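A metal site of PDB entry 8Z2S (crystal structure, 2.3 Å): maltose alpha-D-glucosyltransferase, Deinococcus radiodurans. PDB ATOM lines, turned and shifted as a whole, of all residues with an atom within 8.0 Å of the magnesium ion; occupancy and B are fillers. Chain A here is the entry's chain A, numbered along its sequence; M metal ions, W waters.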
ATOM      1  N   VAL A  21      28.412 -11.075  18.850  1.00  0.00           N
ATOM      2  CA  VAL A  21      28.229  -9.629  18.984  1.00  0.00           C
ATOM      3  C   VAL A  21      28.414  -8.952  17.638  1.00  0.00           C
ATOM      4  O   VAL A  21      27.695  -8.000  17.296  1.00  0.00           O
ATOM      5  CB  VAL A  21      29.203  -9.052  20.044  1.00  0.00           C
ATOM      6  CG1 VAL A  21      29.030  -7.516  20.137  1.00  0.00           C
ATOM      7  CG2 VAL A  21      28.967  -9.676  21.396  1.00  0.00           C
ATOM      8  N   ARG A  22      29.353  -9.475  16.829  1.00  0.00           N
ATOM      9  CA  ARG A  22      29.695  -8.859  15.559  1.00  0.00           C
ATOM     10  C   ARG A  22      28.591  -8.970  14.499  1.00  0.00           C
ATOM     11  O   ARG A  22      28.572  -8.171  13.564  1.00  0.00           O
ATOM     12  CB  ARG A  22      30.982  -9.488  15.018  1.00  0.00           C
ATOM     13  CG  ARG A  22      31.639  -8.672  13.941  1.00  0.00           C
ATOM     14  CD  ARG A  22      33.057  -9.145  13.682  1.00  0.00           C
ATOM     15  NE  ARG A  22      33.996  -8.662  14.686  1.00  0.00           N
ATOM     16  CZ  ARG A  22      34.558  -9.418  15.617  1.00  0.00           C
ATOM     17  NH1 ARG A  22      34.291 -10.706  15.711  1.00  0.00           N
ATOM     18  NH2 ARG A  22      35.428  -8.870  16.463  1.00  0.00           N
ATOM     19  N   GLN A  25      23.588  -6.907  16.351  1.00  0.00           N
ATOM     20  CA  GLN A  25      23.017  -5.578  16.123  1.00  0.00           C
ATOM     21  C   GLN A  25      24.145  -4.548  16.040  1.00  0.00           C
ATOM     22  O   GLN A  25      24.886  -4.361  17.014  1.00  0.00           O
ATOM     23  CB  GLN A  25      22.030  -5.222  17.228  1.00  0.00           C
ATOM     24  CG  GLN A  25      21.542  -3.772  17.153  1.00  0.00           C
ATOM     25  CD  GLN A  25      20.675  -3.562  15.924  1.00  0.00           C
ATOM     26  OE1 GLN A  25      19.598  -4.172  15.805  1.00  0.00           O
ATOM     27  NE2 GLN A  25      21.133  -2.718  14.985  1.00  0.00           N
ATOM     28  N   ASP A  26      24.271  -3.891  14.886  1.00  0.00           N
ATOM     29  CA  ASP A  26      25.211  -2.770  14.785  1.00  0.00           C
ATOM     30  C   ASP A  26      24.657  -1.546  15.503  1.00  0.00           C
ATOM     31  O   ASP A  26      23.489  -1.171  15.307  1.00  0.00           O
ATOM     32  CB  ASP A  26      25.509  -2.445  13.320  1.00  0.00           C
ATOM     33  CG  ASP A  26      26.506  -1.308  13.148  1.00  0.00           C
ATOM     34  OD1 ASP A  26      27.111  -0.890  14.158  1.00  0.00           O
ATOM     35  OD2 ASP A  26      26.704  -0.844  12.007  1.00  0.00           O
ATOM     36  N   GLY A  27      25.465  -0.933  16.345  1.00  0.00           N
ATOM     37  CA  GLY A  27      24.971   0.174  17.146  1.00  0.00           C
ATOM     38  C   GLY A  27      25.528   1.520  16.745  1.00  0.00           C
ATOM     39  O   GLY A  27      25.091   2.548  17.272  1.00  0.00           O
ATOM     40  N   ASN A  28      26.501   1.556  15.811  1.00  0.00           N
ATOM     41  CA  ASN A  28      27.180   2.813  15.512  1.00  0.00           C
ATOM     42  C   ASN A  28      27.416   3.059  14.024  1.00  0.00           C
ATOM     43  O   ASN A  28      28.201   3.951  13.681  1.00  0.00           O
ATOM     44  CB  ASN A  28      28.512   2.870  16.241  1.00  0.00           C
ATOM     45  CG  ASN A  28      29.519   1.888  15.679  1.00  0.00           C
ATOM     46  OD1 ASN A  28      29.160   0.897  15.063  1.00  0.00           O
ATOM     47  ND2 ASN A  28      30.792   2.164  15.883  1.00  0.00           N
ATOM     48  N   GLY A  29      26.800   2.290  13.133  1.00  0.00           N
ATOM     49  CA  GLY A  29      26.779   2.615  11.718  1.00  0.00           C
ATOM     50  C   GLY A  29      27.952   2.136  10.898  1.00  0.00           C
ATOM     51  O   GLY A  29      28.008   2.449   9.718  1.00  0.00           O
ATOM     52  N   ASP A  30      28.893   1.366  11.464  1.00  0.00           N
ATOM     53  CA  ASP A  30      30.075   0.914  10.748  1.00  0.00           C
ATOM     54  C   ASP A  30      29.920  -0.465  10.098  1.00  0.00           C
ATOM     55  O   ASP A  30      30.874  -0.975   9.509  1.00  0.00           O
ATOM     56  CB  ASP A  30      31.300   0.900  11.681  1.00  0.00           C
ATOM     57  CG  ASP A  30      31.286  -0.267  12.658  1.00  0.00           C
ATOM     58  OD1 ASP A  30      30.186  -0.831  12.934  1.00  0.00           O
ATOM     59  OD2 ASP A  30      32.382  -0.618  13.158  1.00  0.00           O
ATOM     60  N   GLY A  31      28.740  -1.086  10.217  1.00  0.00           N
ATOM     61  CA  GLY A  31      28.540  -2.379   9.590  1.00  0.00           C
ATOM     62  C   GLY A  31      29.028  -3.570  10.383  1.00  0.00           C
ATOM     63  O   GLY A  31      29.017  -4.688   9.847  1.00  0.00           O
ATOM     64  N   LYS A  32      29.443  -3.374  11.628  1.00  0.00           N
ATOM     65  CA  LYS A  32      29.843  -4.438  12.531  1.00  0.00           C
ATOM     66  C   LYS A  32      28.986  -4.372  13.778  1.00  0.00           C
ATOM     67  O   LYS A  32      28.718  -3.283  14.296  1.00  0.00           O
ATOM     68  CB  LYS A  32      31.319  -4.346  12.920  1.00  0.00           C
ATOM     69  CG  LYS A  32      32.285  -4.465  11.735  1.00  0.00           C
ATOM     70  CD  LYS A  32      33.684  -4.023  12.097  1.00  0.00           C
ATOM     71  CE  LYS A  32      34.460  -3.579  10.866  1.00  0.00           C
ATOM     72  NZ  LYS A  32      35.922  -3.441  11.189  1.00  0.00           N
ATOM     73  N   GLY A  33      28.544  -5.540  14.243  1.00  0.00           N
ATOM     74  CA  GLY A  33      27.825  -5.587  15.500  1.00  0.00           C
ATOM     75  C   GLY A  33      28.708  -5.191  16.667  1.00  0.00           C
ATOM     76  O   GLY A  33      29.919  -5.425  16.665  1.00  0.00           O
ATOM     77  N   ASP A  34      28.107  -4.579  17.682  1.00  0.00           N
ATOM     78  CA  ASP A  34      28.856  -4.122  18.848  1.00  0.00           C
ATOM     79  C   ASP A  34      28.013  -4.334  20.091  1.00  0.00           C
ATOM     80  O   ASP A  34      26.821  -4.668  20.019  1.00  0.00           O
ATOM     81  CB  ASP A  34      29.267  -2.656  18.741  1.00  0.00           C
ATOM     82  CG  ASP A  34      28.142  -1.779  18.172  1.00  0.00           C
ATOM     83  OD1 ASP A  34      27.059  -1.698  18.802  1.00  0.00           O
ATOM     84  OD2 ASP A  34      28.339  -1.169  17.095  1.00  0.00           O
ATOM     85  N   PHE A  35      28.655  -4.118  21.244  1.00  0.00           N
ATOM     86  CA  PHE A  35      27.973  -4.312  22.515  1.00  0.00           C
ATOM     87  C   PHE A  35      26.901  -3.266  22.790  1.00  0.00           C
ATOM     88  O   PHE A  35      25.884  -3.603  23.415  1.00  0.00           O
ATOM     89  CB  PHE A  35      28.982  -4.327  23.673  1.00  0.00           C
ATOM     90  CG  PHE A  35      29.605  -5.662  23.891  1.00  0.00           C
ATOM     91  CD1 PHE A  35      28.877  -6.673  24.482  1.00  0.00           C
ATOM     92  CD2 PHE A  35      30.899  -5.920  23.490  1.00  0.00           C
ATOM     93  CE1 PHE A  35      29.433  -7.920  24.693  1.00  0.00           C
ATOM     94  CE2 PHE A  35      31.471  -7.160  23.688  1.00  0.00           C
ATOM     95  CZ  PHE A  35      30.733  -8.166  24.298  1.00  0.00           C
ATOM     96  N   PRO A  36      27.042  -2.004  22.370  1.00  0.00           N
ATOM     97  CA  PRO A  36      25.901  -1.097  22.492  1.00  0.00           C
ATOM     98  C   PRO A  36      24.679  -1.550  21.693  1.00  0.00           C
ATOM     99  O   PRO A  36      23.545  -1.406  22.180  1.00  0.00           O
ATOM    100  CB  PRO A  36      26.470   0.245  21.990  1.00  0.00           C
ATOM    101  CG  PRO A  36      27.909   0.145  22.325  1.00  0.00           C
ATOM    102  CD  PRO A  36      28.282  -1.261  22.068  1.00  0.00           C
ATOM    103  N   GLY A  37      24.893  -2.095  20.487  1.00  0.00           N
ATOM    104  CA  GLY A  37      23.779  -2.650  19.710  1.00  0.00           C
ATOM    105  C   GLY A  37      23.135  -3.837  20.401  1.00  0.00           C
ATOM    106  O   GLY A  37      21.909  -3.955  20.463  1.00  0.00           O
ATOM    107  N   PRO A  78      38.248  -4.228  19.138  1.00  0.00           N
ATOM    108  CA  PRO A  78      37.800  -2.849  18.841  1.00  0.00           C
ATOM    109  C   PRO A  78      36.466  -2.767  18.109  1.00  0.00           C
ATOM    110  O   PRO A  78      35.663  -1.880  18.420  1.00  0.00           O
ATOM    111  CB  PRO A  78      38.932  -2.295  17.983  1.00  0.00           C
ATOM    112  CG  PRO A  78      40.137  -3.076  18.412  1.00  0.00           C
ATOM    113  CD  PRO A  78      39.658  -4.456  18.775  1.00  0.00           C
ATOM    114  N   ASP A  79      36.212  -3.653  17.150  1.00  0.00           N
ATOM    115  CA  ASP A  79      34.922  -3.671  16.439  1.00  0.00           C
ATOM    116  C   ASP A  79      33.748  -3.550  17.396  1.00  0.00           C
ATOM    117  O   ASP A  79      32.809  -2.798  17.151  1.00  0.00           O
ATOM    118  CB  ASP A  79      34.756  -4.958  15.636  1.00  0.00           C
ATOM    119  CG  ASP A  79      35.801  -5.109  14.557  1.00  0.00           C
ATOM    120  OD1 ASP A  79      36.515  -4.106  14.300  1.00  0.00           O
ATOM    121  OD2 ASP A  79      35.901  -6.245  14.003  1.00  0.00           O
ATOM    122  N   LEU A  80      33.821  -4.265  18.514  1.00  0.00           N
ATOM    123  CA  LEU A  80      32.657  -4.489  19.364  1.00  0.00           C
ATOM    124  C   LEU A  80      32.426  -3.387  20.403  1.00  0.00           C
ATOM    125  O   LEU A  80      31.441  -3.466  21.135  1.00  0.00           O
ATOM    126  CB  LEU A  80      32.820  -5.847  20.062  1.00  0.00           C
ATOM    127  CG  LEU A  80      33.310  -6.941  19.099  1.00  0.00           C
ATOM    128  CD1 LEU A  80      33.447  -8.254  19.824  1.00  0.00           C
ATOM    129  CD2 LEU A  80      32.413  -7.129  17.849  1.00  0.00           C
ATOM    130  N   GLY A  81      33.283  -2.369  20.458  1.00  0.00           N
ATOM    131  CA  GLY A  81      33.197  -1.369  21.513  1.00  0.00           C
ATOM    132  C   GLY A  81      34.317  -1.521  22.524  1.00  0.00           C
ATOM    133  O   GLY A  81      35.404  -2.029  22.182  1.00  0.00           O
ATOM    134  N   PHE A 417      19.914  -4.474  10.846  1.00  0.00           N
ATOM    135  CA  PHE A 417      21.130  -4.787  11.594  1.00  0.00           C
ATOM    136  C   PHE A 417      22.039  -3.577  11.706  1.00  0.00           C
ATOM    137  O   PHE A 417      22.766  -3.432  12.704  1.00  0.00           O
ATOM    138  CB  PHE A 417      21.833  -5.983  10.932  1.00  0.00           C
ATOM    139  CG  PHE A 417      23.300  -6.066  11.190  1.00  0.00           C
ATOM    140  CD1 PHE A 417      23.794  -6.642  12.354  1.00  0.00           C
ATOM    141  CD2 PHE A 417      24.203  -5.616  10.238  1.00  0.00           C
ATOM    142  CE1 PHE A 417      25.163  -6.735  12.600  1.00  0.00           C
ATOM    143  CE2 PHE A 417      25.576  -5.708  10.461  1.00  0.00           C
ATOM    144  CZ  PHE A 417      26.059  -6.279  11.644  1.00  0.00           C
ATOM    145  N   SER A 418      21.955  -2.665  10.750  1.00  0.00           N
ATOM    146  CA  SER A 418      22.911  -1.583  10.559  1.00  0.00           C
ATOM    147  C   SER A 418      22.266  -0.518   9.697  1.00  0.00           C
ATOM    148  O   SER A 418      21.378  -0.833   8.906  1.00  0.00           O
ATOM    149  CB  SER A 418      24.186  -2.097   9.873  1.00  0.00           C
ATOM    150  OG  SER A 418      25.050  -1.023   9.563  1.00  0.00           O
HETATM  151 MG    MG M   1      29.260  -1.184  14.997  1.00  0.00          MG
HETATM  152  O   HOH W   1      31.451  -0.285  16.674  1.00  0.00           O
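The magnesium ion is bound by OD1 of Asn 28 (2.1 Å), O of Lys 32 (2.3 Å), OD1 of Asp 30 (2.3 Å), OD2 of Asp 34 (2.3 Å) and OD1 of Asp 26 (2.3 Å).
The magnesium ion has five donor atoms within binding distance.
Five residues have an atom within 4 Å of the magnesium ion: Asp 26, Asn 28, Asp 30, Lys 32 and Asp 34.
OD1 of Asp 34 sits at hydrogen-bond distance from N of Gly 27.
The backbone NH (N) of Asp 34 lies within hydrogen-bond range of the backbone carbonyl oxygen (O) of Gln 25 (3.3 Å).
The side-chain carboxylate (OD1) of Asp 34 sits at hydrogen-bond distance from the backbone NH (N) of Gly 37, at 2.8 Å.
O of Val 21 is in hydrogen-bond range of N of Asp 34.
The backbone NH (N) of Gly 29 sits at hydrogen-bond distance from the side-chain carboxylate (OD2) of Asp 26 (3.3 Å).
The side-chain carboxylate of Asp 26 is in hydrogen-bond range of the backbone NH of Gly 31.
The side-chain hydroxyl (OG) of Ser 418 sits at hydrogen-bond distance from the side-chain carboxylate (OD2) of Asp 26, at 3.0 Å.
O of Phe 417 sits at hydrogen-bond distance from N of Asp 26.
Water W1 bridges ND2 of Asn 28 (2.7 Å) and O of Asp 79 (2.9 Å).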
